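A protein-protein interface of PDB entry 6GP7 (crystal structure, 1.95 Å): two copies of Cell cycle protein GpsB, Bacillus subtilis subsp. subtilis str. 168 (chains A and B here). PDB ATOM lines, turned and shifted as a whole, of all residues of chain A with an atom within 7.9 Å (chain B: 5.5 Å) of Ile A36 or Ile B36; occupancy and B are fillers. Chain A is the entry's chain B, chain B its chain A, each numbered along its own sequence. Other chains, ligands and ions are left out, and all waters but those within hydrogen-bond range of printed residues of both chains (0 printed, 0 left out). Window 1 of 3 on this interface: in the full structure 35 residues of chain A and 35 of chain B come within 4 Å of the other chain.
CE of Met B35 touches CE of Lys A6 (3.6 Å). Phe B32 touches Leu A7 (CZ to CD1, 3.6 Å). Ile B36 touches Leu A7 (CG1 to CD1, 3.7 Å). Ile B36 touches Ile A12. CZ of Phe A32 touches CD1 of Leu B7, 3.7 Å away. Ile B12 touches Phe A32 (CA to CZ, 3.96 Å). CB of Met A35 touches CD1 of Leu B7, at 3.9 Å. Leu B7 touches Ile A36. Ile A36 touches Ile B36 (CG2 to CG2, 3.7 Å). CE2 of Phe A43 touches CD2 of Tyr B40 (3.6 Å).
N of Lys A6 is in hydrogen-bond range of OD1 of Asp B39 (2.8 Å). The backbone NH (N) of Leu A7 lies within hydrogen-bond range of the side-chain carboxylate (OD2) of Asp B39, 2.8 Å away. OD2 of Asp A39 sits at hydrogen-bond distance from N of Leu B7 (2.8 Å). The side-chain carboxylate of Asp A39 is in hydrogen-bond range of the side-chain hydroxyl of Tyr B40 (2.5 Å). The side-chain hydroxyl of Tyr A40 is in hydrogen-bond range of the side-chain carboxylate of Asp B39 (2.6 Å).
Of the printed residues of chain B, Ile A12 touches Phe B32 and Ile B36. Printed residues of chain B within 4 Å of Phe A17: Phe B32. Of chain B, only Leu B7, Ile B36 and Tyr B40 come within 4 Å of Ile A36. Glu A41 touches none of the printed residues of chain B. Printed residues of chain A within 4 Å of Ile B36: Leu A7 (3.7 Å), Ile A12 (3.99 Å), Leu A33 (3.7 Å), Ile A36 (3.7 Å) and Tyr A40 (3.7 Å).
Leu A7 touches Ile B36, and with the chains exchanged Ile A36 touches Leu B7. Ile A12 touches Phe B32, and with the chains exchanged Phe A32 touches Ile B12. Ile A12 touches Ile B36, but with the chains exchanged Ile A36 does not touch Ile B12 (4.3 Å). Asp A39 touches Tyr B40, and with the chains exchanged Tyr A40 touches Asp B39.
Hydrophobic or aromatic side chains of chain B within 4 Å of the printed part of chain A: Leu B7, Phe B32, Met B35, Ile B36 and Tyr B40. Hydrophobic or aromatic side chains of chain A that line the printed part of chain B: Val A5, Leu A7, Ile A12, Phe A17, Phe A32, Leu A33, Met A35, Ile A36, Tyr A40 and Phe A43.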
ATOM      1  N   VAL A   5       0.412  -1.549   2.089  1.00  0.00           N
ATOM      2  CA  VAL A   5       1.549  -2.161   1.415  1.00  0.00           C
ATOM      3  C   VAL A   5       2.823  -1.817   2.174  1.00  0.00           C
ATOM      4  O   VAL A   5       3.026  -0.675   2.596  1.00  0.00           O
ATOM      5  CB  VAL A   5       1.604  -1.697  -0.048  1.00  0.00           C
ATOM      6  CG1 VAL A   5       2.913  -2.054  -0.675  1.00  0.00           C
ATOM      7  CG2 VAL A   5       0.467  -2.340  -0.822  1.00  0.00           C
ATOM      8  N   LYS A   6       3.682  -2.809   2.370  1.00  0.00           N
ATOM      9  CA  LYS A   6       4.847  -2.599   3.219  1.00  0.00           C
ATOM     10  C   LYS A   6       6.045  -2.066   2.442  1.00  0.00           C
ATOM     11  O   LYS A   6       6.763  -1.192   2.933  1.00  0.00           O
ATOM     12  CB  LYS A   6       5.198  -3.904   3.926  1.00  0.00           C
ATOM     13  CG  LYS A   6       4.004  -4.476   4.680  1.00  0.00           C
ATOM     14  CD  LYS A   6       4.190  -5.933   5.029  1.00  0.00           C
ATOM     15  CE  LYS A   6       5.278  -6.107   6.070  1.00  0.00           C
ATOM     16  NZ  LYS A   6       5.007  -5.296   7.291  1.00  0.00           N
ATOM     17  N   LEU A   7       6.270  -2.563   1.237  1.00  0.00           N
ATOM     18  CA  LEU A   7       7.406  -2.145   0.436  1.00  0.00           C
ATOM     19  C   LEU A   7       6.942  -1.273  -0.727  1.00  0.00           C
ATOM     20  O   LEU A   7       5.752  -1.013  -0.918  1.00  0.00           O
ATOM     21  CB  LEU A   7       8.187  -3.368  -0.055  1.00  0.00           C
ATOM     22  CG  LEU A   7       8.839  -4.188   1.060  1.00  0.00           C
ATOM     23  CD1 LEU A   7       9.541  -5.406   0.493  1.00  0.00           C
ATOM     24  CD2 LEU A   7       9.823  -3.322   1.828  1.00  0.00           C
ATOM     25  N   SER A   8       7.916  -0.794  -1.489  1.00  0.00           N
ATOM     26  CA  SER A   8       7.689  -0.048  -2.715  1.00  0.00           C
ATOM     27  C   SER A   8       8.716  -0.522  -3.726  1.00  0.00           C
ATOM     28  O   SER A   8       9.688  -1.194  -3.375  1.00  0.00           O
ATOM     29  CB  SER A   8       7.809   1.456  -2.497  1.00  0.00           C
ATOM     30  OG  SER A   8       9.119   1.802  -2.092  1.00  0.00           O
ATOM     31  N   ALA A   9       8.492  -0.172  -4.993  1.00  0.00           N
ATOM     32  CA  ALA A   9       9.463  -0.510  -6.028  1.00  0.00           C
ATOM     33  C   ALA A   9      10.826   0.104  -5.723  1.00  0.00           C
ATOM     34  O   ALA A   9      11.862  -0.553  -5.883  1.00  0.00           O
ATOM     35  CB  ALA A   9       8.949  -0.048  -7.388  1.00  0.00           C
ATOM     36  N   ILE A  12      12.608  -1.829  -2.906  1.00  0.00           N
ATOM     37  CA  ILE A  12      13.149  -3.102  -3.382  1.00  0.00           C
ATOM     38  C   ILE A  12      14.374  -2.870  -4.268  1.00  0.00           C
ATOM     39  O   ILE A  12      15.354  -3.618  -4.200  1.00  0.00           O
ATOM     40  CB  ILE A  12      12.049  -3.904  -4.096  1.00  0.00           C
ATOM     41  CG1 ILE A  12      10.949  -4.249  -3.088  1.00  0.00           C
ATOM     42  CG2 ILE A  12      12.618  -5.192  -4.701  1.00  0.00           C
ATOM     43  CD1 ILE A  12       9.721  -4.921  -3.696  1.00  0.00           C
ATOM     44  N   PHE A  17      21.292  -6.460   0.801  1.00  0.00           N
ATOM     45  CA  PHE A  17      21.383  -7.635   1.655  1.00  0.00           C
ATOM     46  C   PHE A  17      22.821  -7.834   2.109  1.00  0.00           C
ATOM     47  O   PHE A  17      23.757  -7.688   1.317  1.00  0.00           O
ATOM     48  CB  PHE A  17      20.946  -8.899   0.911  1.00  0.00           C
ATOM     49  CG  PHE A  17      19.543  -8.843   0.408  1.00  0.00           C
ATOM     50  CD1 PHE A  17      18.488  -8.988   1.278  1.00  0.00           C
ATOM     51  CD2 PHE A  17      19.280  -8.658  -0.938  1.00  0.00           C
ATOM     52  CE1 PHE A  17      17.189  -8.927   0.816  1.00  0.00           C
ATOM     53  CE2 PHE A  17      17.987  -8.589  -1.397  1.00  0.00           C
ATOM     54  CZ  PHE A  17      16.946  -8.733  -0.511  1.00  0.00           C
ATOM     55  N   VAL A  29      19.228 -13.642  -7.385  1.00  0.00           N
ATOM     56  CA  VAL A  29      18.311 -12.866  -6.553  1.00  0.00           C
ATOM     57  C   VAL A  29      17.999 -11.525  -7.207  1.00  0.00           C
ATOM     58  O   VAL A  29      16.851 -11.061  -7.179  1.00  0.00           O
ATOM     59  CB  VAL A  29      18.894 -12.675  -5.136  1.00  0.00           C
ATOM     60  CG1 VAL A  29      18.085 -11.626  -4.342  1.00  0.00           C
ATOM     61  CG2 VAL A  29      18.887 -13.986  -4.364  1.00  0.00           C
ATOM     62  N   ASP A  30      19.004 -10.872  -7.801  1.00  0.00           N
ATOM     63  CA  ASP A  30      18.770  -9.528  -8.323  1.00  0.00           C
ATOM     64  C   ASP A  30      17.928  -9.558  -9.589  1.00  0.00           C
ATOM     65  O   ASP A  30      17.108  -8.654  -9.813  1.00  0.00           O
ATOM     66  CB  ASP A  30      20.096  -8.808  -8.577  1.00  0.00           C
ATOM     67  CG  ASP A  30      20.770  -8.387  -7.278  1.00  0.00           C
ATOM     68  OD1 ASP A  30      20.063  -8.227  -6.258  1.00  0.00           O
ATOM     69  OD2 ASP A  30      21.998  -8.225  -7.271  1.00  0.00           O
ATOM     70  N   LYS A  31      18.122 -10.569 -10.446  1.00  0.00           N
ATOM     71  CA  LYS A  31      17.259 -10.686 -11.618  1.00  0.00           C
ATOM     72  C   LYS A  31      15.818 -10.986 -11.221  1.00  0.00           C
ATOM     73  O   LYS A  31      14.882 -10.508 -11.879  1.00  0.00           O
ATOM     74  CB  LYS A  31      17.779 -11.767 -12.568  1.00  0.00           C
ATOM     75  CG  LYS A  31      18.952 -11.297 -13.423  1.00  0.00           C
ATOM     76  CD  LYS A  31      19.423 -12.358 -14.405  1.00  0.00           C
ATOM     77  CE  LYS A  31      20.625 -11.847 -15.204  1.00  0.00           C
ATOM     78  NZ  LYS A  31      21.297 -12.911 -15.996  1.00  0.00           N
ATOM     79  N   PHE A  32      15.623 -11.777 -10.166  1.00  0.00           N
ATOM     80  CA  PHE A  32      14.275 -12.092  -9.695  1.00  0.00           C
ATOM     81  C   PHE A  32      13.604 -10.874  -9.068  1.00  0.00           C
ATOM     82  O   PHE A  32      12.415 -10.620  -9.302  1.00  0.00           O
ATOM     83  CB  PHE A  32      14.341 -13.227  -8.685  1.00  0.00           C
ATOM     84  CG  PHE A  32      13.015 -13.874  -8.431  1.00  0.00           C
ATOM     85  CD1 PHE A  32      12.393 -14.616  -9.428  1.00  0.00           C
ATOM     86  CD2 PHE A  32      12.386 -13.740  -7.203  1.00  0.00           C
ATOM     87  CE1 PHE A  32      11.167 -15.229  -9.204  1.00  0.00           C
ATOM     88  CE2 PHE A  32      11.155 -14.345  -6.974  1.00  0.00           C
ATOM     89  CZ  PHE A  32      10.544 -15.084  -7.978  1.00  0.00           C
ATOM     90  N   LEU A  33      14.347 -10.108  -8.265  1.00  0.00           N
ATOM     91  CA  LEU A  33      13.762  -8.917  -7.654  1.00  0.00           C
ATOM     92  C   LEU A  33      13.482  -7.830  -8.686  1.00  0.00           C
ATOM     93  O   LEU A  33      12.593  -7.007  -8.470  1.00  0.00           O
ATOM     94  CB  LEU A  33      14.682  -8.367  -6.559  1.00  0.00           C
ATOM     95  CG  LEU A  33      14.719  -9.090  -5.207  1.00  0.00           C
ATOM     96  CD1 LEU A  33      15.708  -8.391  -4.305  1.00  0.00           C
ATOM     97  CD2 LEU A  33      13.366  -9.118  -4.548  1.00  0.00           C
ATOM     98  N   ASP A  34      14.238  -7.787  -9.792  1.00  0.00           N
ATOM     99  CA  ASP A  34      13.925  -6.839 -10.863  1.00  0.00           C
ATOM    100  C   ASP A  34      12.568  -7.141 -11.491  1.00  0.00           C
ATOM    101  O   ASP A  34      11.866  -6.231 -11.942  1.00  0.00           O
ATOM    102  CB  ASP A  34      15.012  -6.860 -11.943  1.00  0.00           C
ATOM    103  CG  ASP A  34      16.240  -6.023 -11.573  1.00  0.00           C
ATOM    104  OD1 ASP A  34      16.126  -5.117 -10.718  1.00  0.00           O
ATOM    105  OD2 ASP A  34      17.322  -6.275 -12.153  1.00  0.00           O
ATOM    106  N   MET A  35      12.194  -8.414 -11.567  1.00  0.00           N
ATOM    107  CA  MET A  35      10.854  -8.726 -12.055  1.00  0.00           C
ATOM    108  C   MET A  35       9.796  -8.303 -11.049  1.00  0.00           C
ATOM    109  O   MET A  35       8.744  -7.785 -11.430  1.00  0.00           O
ATOM    110  CB  MET A  35      10.736 -10.212 -12.354  1.00  0.00           C
ATOM    111  CG  MET A  35      11.450 -10.623 -13.610  1.00  0.00           C
ATOM    112  SD  MET A  35      10.959 -12.286 -14.050  1.00  0.00           S
ATOM    113  CE  MET A  35      11.813 -13.195 -12.800  1.00  0.00           C
ATOM    114  N   ILE A  36      10.060  -8.515  -9.760  1.00  0.00           N
ATOM    115  CA  ILE A  36       9.142  -8.059  -8.720  1.00  0.00           C
ATOM    116  C   ILE A  36       8.985  -6.538  -8.766  1.00  0.00           C
ATOM    117  O   ILE A  36       7.880  -6.007  -8.588  1.00  0.00           O
ATOM    118  CB  ILE A  36       9.626  -8.553  -7.344  1.00  0.00           C
ATOM    119  CG1 ILE A  36       9.497 -10.077  -7.243  1.00  0.00           C
ATOM    120  CG2 ILE A  36       8.864  -7.863  -6.200  1.00  0.00           C
ATOM    121  CD1 ILE A  36      10.156 -10.666  -6.021  1.00  0.00           C
ATOM    122  N   ILE A  37      10.082  -5.815  -9.017  1.00  0.00           N
ATOM    123  CA  ILE A  37      10.016  -4.357  -9.106  1.00  0.00           C
ATOM    124  C   ILE A  37       9.090  -3.924 -10.239  1.00  0.00           C
ATOM    125  O   ILE A  37       8.301  -2.983 -10.088  1.00  0.00           O
ATOM    126  CB  ILE A  37      11.428  -3.766  -9.286  1.00  0.00           C
ATOM    127  CG1 ILE A  37      12.191  -3.797  -7.960  1.00  0.00           C
ATOM    128  CG2 ILE A  37      11.353  -2.337  -9.791  1.00  0.00           C
ATOM    129  CD1 ILE A  37      13.683  -3.547  -8.123  1.00  0.00           C
ATOM    130  N   LYS A  38       9.190  -4.576 -11.399  1.00  0.00           N
ATOM    131  CA  LYS A  38       8.289  -4.234 -12.495  1.00  0.00           C
ATOM    132  C   LYS A  38       6.844  -4.523 -12.112  1.00  0.00           C
ATOM    133  O   LYS A  38       5.930  -3.778 -12.489  1.00  0.00           O
ATOM    134  CB  LYS A  38       8.667  -5.002 -13.758  1.00  0.00           C
ATOM    135  CG  LYS A  38      10.079  -4.775 -14.262  1.00  0.00           C
ATOM    136  CD  LYS A  38      10.280  -5.450 -15.620  1.00  0.00           C
ATOM    137  CE  LYS A  38      11.734  -5.876 -15.856  1.00  0.00           C
ATOM    138  NZ  LYS A  38      12.166  -7.071 -15.043  1.00  0.00           N
ATOM    139  N   ASP A  39       6.618  -5.606 -11.364  1.00  0.00           N
ATOM    140  CA  ASP A  39       5.267  -5.930 -10.908  1.00  0.00           C
ATOM    141  C   ASP A  39       4.721  -4.855  -9.977  1.00  0.00           C
ATOM    142  O   ASP A  39       3.558  -4.463 -10.100  1.00  0.00           O
ATOM    143  CB  ASP A  39       5.242  -7.291 -10.205  1.00  0.00           C
ATOM    144  CG  ASP A  39       5.216  -8.457 -11.173  1.00  0.00           C
ATOM    145  OD1 ASP A  39       5.064  -8.231 -12.389  1.00  0.00           O
ATOM    146  OD2 ASP A  39       5.343  -9.613 -10.716  1.00  0.00           O
ATOM    147  N   TYR A  40       5.527  -4.386  -9.016  1.00  0.00           N
ATOM    148  CA  TYR A  40       5.049  -3.319  -8.137  1.00  0.00           C
ATOM    149  C   TYR A  40       4.621  -2.104  -8.947  1.00  0.00           C
ATOM    150  O   TYR A  40       3.612  -1.464  -8.632  1.00  0.00           O
ATOM    151  CB  TYR A  40       6.124  -2.900  -7.129  1.00  0.00           C
ATOM    152  CG  TYR A  40       6.117  -3.654  -5.808  1.00  0.00           C
ATOM    153  CD1 TYR A  40       6.394  -5.014  -5.767  1.00  0.00           C
ATOM    154  CD2 TYR A  40       5.888  -2.994  -4.603  1.00  0.00           C
ATOM    155  CE1 TYR A  40       6.417  -5.705  -4.571  1.00  0.00           C
ATOM    156  CE2 TYR A  40       5.904  -3.684  -3.391  1.00  0.00           C
ATOM    157  CZ  TYR A  40       6.176  -5.040  -3.391  1.00  0.00           C
ATOM    158  OH  TYR A  40       6.202  -5.737  -2.219  1.00  0.00           O
ATOM    159  N   GLU A  41       5.391  -1.760  -9.982  1.00  0.00           N
ATOM    160  CA  GLU A  41       5.024  -0.637 -10.836  1.00  0.00           C
ATOM    161  C   GLU A  41       3.714  -0.911 -11.559  1.00  0.00           C
ATOM    162  O   GLU A  41       2.859  -0.025 -11.680  1.00  0.00           O
ATOM    163  CB  GLU A  41       6.156  -0.369 -11.830  1.00  0.00           C
ATOM    164  CG  GLU A  41       7.459   0.057 -11.164  1.00  0.00           C
ATOM    165  CD  GLU A  41       8.649   0.005 -12.105  1.00  0.00           C
ATOM    166  OE1 GLU A  41       8.522  -0.555 -13.219  1.00  0.00           O
ATOM    167  OE2 GLU A  41       9.717   0.528 -11.726  1.00  0.00           O
ATOM    168  N   THR A  42       3.542  -2.139 -12.047  1.00  0.00           N
ATOM    169  CA  THR A  42       2.317  -2.504 -12.752  1.00  0.00           C
ATOM    170  C   THR A  42       1.116  -2.419 -11.820  1.00  0.00           C
ATOM    171  O   THR A  42       0.078  -1.844 -12.175  1.00  0.00           O
ATOM    172  CB  THR A  42       2.461  -3.913 -13.337  1.00  0.00           C
ATOM    173  OG1 THR A  42       3.540  -3.926 -14.283  1.00  0.00           O
ATOM    174  CG2 THR A  42       1.185  -4.346 -14.041  1.00  0.00           C
ATOM    175  N   PHE A  43       1.264  -2.957 -10.608  1.00  0.00           N
ATOM    176  CA  PHE A  43       0.199  -2.926  -9.605  1.00  0.00           C
ATOM    177  C   PHE A  43      -0.221  -1.496  -9.288  1.00  0.00           C
ATOM    178  O   PHE A  43      -1.415  -1.186  -9.223  1.00  0.00           O
ATOM    179  CB  PHE A  43       0.678  -3.620  -8.326  1.00  0.00           C
ATOM    180  CG  PHE A  43       0.591  -5.121  -8.362  1.00  0.00           C
ATOM    181  CD1 PHE A  43      -0.556  -5.756  -8.806  1.00  0.00           C
ATOM    182  CD2 PHE A  43       1.661  -5.893  -7.937  1.00  0.00           C
ATOM    183  CE1 PHE A  43      -0.628  -7.152  -8.834  1.00  0.00           C
ATOM    184  CE2 PHE A  43       1.596  -7.278  -7.946  1.00  0.00           C
ATOM    185  CZ  PHE A  43       0.445  -7.911  -8.407  1.00  0.00           C
ATOM    186  N   LEU B   7       4.927 -12.193 -11.850  1.00  0.00           N
ATOM    187  CA  LEU B   7       5.086 -13.182 -10.796  1.00  0.00           C
ATOM    188  C   LEU B   7       3.802 -13.304  -9.978  1.00  0.00           C
ATOM    189  O   LEU B   7       2.767 -12.722 -10.305  1.00  0.00           O
ATOM    190  CB  LEU B   7       6.299 -12.830  -9.921  1.00  0.00           C
ATOM    191  CG  LEU B   7       7.642 -12.952 -10.643  1.00  0.00           C
ATOM    192  CD1 LEU B   7       8.771 -12.431  -9.766  1.00  0.00           C
ATOM    193  CD2 LEU B   7       7.926 -14.403 -11.084  1.00  0.00           C
ATOM    194  N   ILE B  12       6.815 -16.925  -6.278  1.00  0.00           N
ATOM    195  CA  ILE B  12       7.899 -16.493  -5.397  1.00  0.00           C
ATOM    196  C   ILE B  12       8.276 -17.603  -4.423  1.00  0.00           C
ATOM    197  O   ILE B  12       9.462 -17.840  -4.160  1.00  0.00           O
ATOM    198  CB  ILE B  12       7.501 -15.200  -4.664  1.00  0.00           C
ATOM    199  CG1 ILE B  12       7.372 -14.047  -5.664  1.00  0.00           C
ATOM    200  CG2 ILE B  12       8.517 -14.874  -3.543  1.00  0.00           C
ATOM    201  CD1 ILE B  12       6.510 -12.874  -5.177  1.00  0.00           C
ATOM    202  N   PHE B  32      12.705 -10.925   3.359  1.00  0.00           N
ATOM    203  CA  PHE B  32      12.286  -9.869   2.437  1.00  0.00           C
ATOM    204  C   PHE B  32      11.218 -10.381   1.468  1.00  0.00           C
ATOM    205  O   PHE B  32      10.220  -9.697   1.213  1.00  0.00           O
ATOM    206  CB  PHE B  32      13.509  -9.339   1.669  1.00  0.00           C
ATOM    207  CG  PHE B  32      13.334  -7.948   1.082  1.00  0.00           C
ATOM    208  CD1 PHE B  32      13.184  -6.849   1.906  1.00  0.00           C
ATOM    209  CD2 PHE B  32      13.372  -7.743  -0.300  1.00  0.00           C
ATOM    210  CE1 PHE B  32      13.042  -5.567   1.368  1.00  0.00           C
ATOM    211  CE2 PHE B  32      13.236  -6.463  -0.841  1.00  0.00           C
ATOM    212  CZ  PHE B  32      13.074  -5.380  -0.007  1.00  0.00           C
ATOM    213  N   LEU B  33      11.417 -11.584   0.928  1.00  0.00           N
ATOM    214  CA  LEU B  33      10.439 -12.194   0.036  1.00  0.00           C
ATOM    215  C   LEU B  33       9.107 -12.436   0.735  1.00  0.00           C
ATOM    216  O   LEU B  33       8.058 -12.417   0.084  1.00  0.00           O
ATOM    217  CB  LEU B  33      10.988 -13.516  -0.517  1.00  0.00           C
ATOM    218  CG  LEU B  33      12.195 -13.385  -1.475  1.00  0.00           C
ATOM    219  CD1 LEU B  33      12.682 -14.744  -1.912  1.00  0.00           C
ATOM    220  CD2 LEU B  33      11.844 -12.570  -2.718  1.00  0.00           C
ATOM    221  N   ASP B  34       9.133 -12.710   2.041  1.00  0.00           N
ATOM    222  CA  ASP B  34       7.896 -12.900   2.801  1.00  0.00           C
ATOM    223  C   ASP B  34       7.057 -11.619   2.833  1.00  0.00           C
ATOM    224  O   ASP B  34       5.825 -11.663   2.725  1.00  0.00           O
ATOM    225  CB  ASP B  34       8.243 -13.350   4.220  1.00  0.00           C
ATOM    226  CG  ASP B  34       7.043 -13.341   5.149  1.00  0.00           C
ATOM    227  OD1 ASP B  34       6.163 -14.189   4.937  1.00  0.00           O
ATOM    228  OD2 ASP B  34       6.984 -12.513   6.095  1.00  0.00           O
ATOM    229  N   MET B  35       7.706 -10.469   3.001  1.00  0.00           N
ATOM    230  CA  MET B  35       6.995  -9.195   2.931  1.00  0.00           C
ATOM    231  C   MET B  35       6.461  -8.938   1.530  1.00  0.00           C
ATOM    232  O   MET B  35       5.346  -8.428   1.371  1.00  0.00           O
ATOM    233  CB  MET B  35       7.916  -8.052   3.345  1.00  0.00           C
ATOM    234  CG  MET B  35       8.378  -8.109   4.780  1.00  0.00           C
ATOM    235  SD  MET B  35       9.454  -6.709   5.138  1.00  0.00           S
ATOM    236  CE  MET B  35       8.469  -5.340   4.547  1.00  0.00           C
ATOM    237  N   ILE B  36       7.242  -9.285   0.504  1.00  0.00           N
ATOM    238  CA  ILE B  36       6.805  -9.086  -0.876  1.00  0.00           C
ATOM    239  C   ILE B  36       5.571  -9.926  -1.178  1.00  0.00           C
ATOM    240  O   ILE B  36       4.641  -9.470  -1.859  1.00  0.00           O
ATOM    241  CB  ILE B  36       7.953  -9.407  -1.848  1.00  0.00           C
ATOM    242  CG1 ILE B  36       9.047  -8.341  -1.753  1.00  0.00           C
ATOM    243  CG2 ILE B  36       7.431  -9.554  -3.290  1.00  0.00           C
ATOM    244  CD1 ILE B  36      10.345  -8.754  -2.423  1.00  0.00           C
ATOM    245  N   ILE B  37       5.550 -11.171  -0.694  1.00  0.00           N
ATOM    246  CA  ILE B  37       4.381 -12.035  -0.891  1.00  0.00           C
ATOM    247  C   ILE B  37       3.147 -11.415  -0.254  1.00  0.00           C
ATOM    248  O   ILE B  37       2.040 -11.477  -0.806  1.00  0.00           O
ATOM    249  CB  ILE B  37       4.653 -13.438  -0.319  1.00  0.00           C
ATOM    250  CG1 ILE B  37       5.615 -14.193  -1.226  1.00  0.00           C
ATOM    251  CG2 ILE B  37       3.347 -14.229  -0.135  1.00  0.00           C
ATOM    252  CD1 ILE B  37       6.164 -15.445  -0.596  1.00  0.00           C
ATOM    253  N   LYS B  38       3.307 -10.848   0.935  1.00  0.00           N
ATOM    254  CA  LYS B  38       2.175 -10.199   1.586  1.00  0.00           C
ATOM    255  C   LYS B  38       1.708  -8.994   0.781  1.00  0.00           C
ATOM    256  O   LYS B  38       0.508  -8.730   0.690  1.00  0.00           O
ATOM    257  CB  LYS B  38       2.552  -9.791   3.009  1.00  0.00           C
ATOM    258  CG  LYS B  38       2.587 -10.950   4.011  1.00  0.00           C
ATOM    259  CD  LYS B  38       3.150 -10.510   5.355  1.00  0.00           C
ATOM    260  CE  LYS B  38       3.369 -11.698   6.290  1.00  0.00           C
ATOM    261  NZ  LYS B  38       4.423 -11.408   7.310  1.00  0.00           N
ATOM    262  N   ASP B  39       2.643  -8.266   0.171  1.00  0.00           N
ATOM    263  CA  ASP B  39       2.261  -7.137  -0.672  1.00  0.00           C
ATOM    264  C   ASP B  39       1.512  -7.596  -1.925  1.00  0.00           C
ATOM    265  O   ASP B  39       0.549  -6.942  -2.345  1.00  0.00           O
ATOM    266  CB  ASP B  39       3.504  -6.319  -1.045  1.00  0.00           C
ATOM    267  CG  ASP B  39       3.963  -5.369   0.074  1.00  0.00           C
ATOM    268  OD1 ASP B  39       3.255  -5.217   1.098  1.00  0.00           O
ATOM    269  OD2 ASP B  39       5.043  -4.749  -0.080  1.00  0.00           O
ATOM    270  N   TYR B  40       1.918  -8.716  -2.541  1.00  0.00           N
ATOM    271  CA  TYR B  40       1.172  -9.198  -3.707  1.00  0.00           C
ATOM    272  C   TYR B  40      -0.281  -9.478  -3.341  1.00  0.00           C
ATOM    273  O   TYR B  40      -1.199  -9.191  -4.122  1.00  0.00           O
ATOM    274  CB  TYR B  40       1.815 -10.457  -4.296  1.00  0.00           C
ATOM    275  CG  TYR B  40       2.858 -10.215  -5.380  1.00  0.00           C
ATOM    276  CD1 TYR B  40       4.116  -9.729  -5.056  1.00  0.00           C
ATOM    277  CD2 TYR B  40       2.598 -10.522  -6.714  1.00  0.00           C
ATOM    278  CE1 TYR B  40       5.083  -9.521  -6.028  1.00  0.00           C
ATOM    279  CE2 TYR B  40       3.576 -10.324  -7.702  1.00  0.00           C
ATOM    280  CZ  TYR B  40       4.814  -9.820  -7.338  1.00  0.00           C
ATOM    281  OH  TYR B  40       5.805  -9.613  -8.268  1.00  0.00           O
ATOM    282  N   GLU B  41      -0.508 -10.034  -2.155  1.00  0.00           N
ATOM    283  CA  GLU B  41      -1.872 -10.276  -1.690  1.00  0.00           C
ATOM    284  C   GLU B  41      -2.638  -8.968  -1.532  1.00  0.00           C
ATOM    285  O   GLU B  41      -3.795  -8.851  -1.957  1.00  0.00           O
ATOM    286  CB  GLU B  41      -1.832 -11.044  -0.370  1.00  0.00           C
ATOM    287  CG  GLU B  41      -3.176 -11.094   0.338  1.00  0.00           C
ATOM    288  CD  GLU B  41      -3.099 -11.730   1.720  1.00  0.00           C
ATOM    289  OE1 GLU B  41      -1.994 -12.167   2.122  1.00  0.00           O
ATOM    290  OE2 GLU B  41      -4.148 -11.788   2.402  1.00  0.00           O
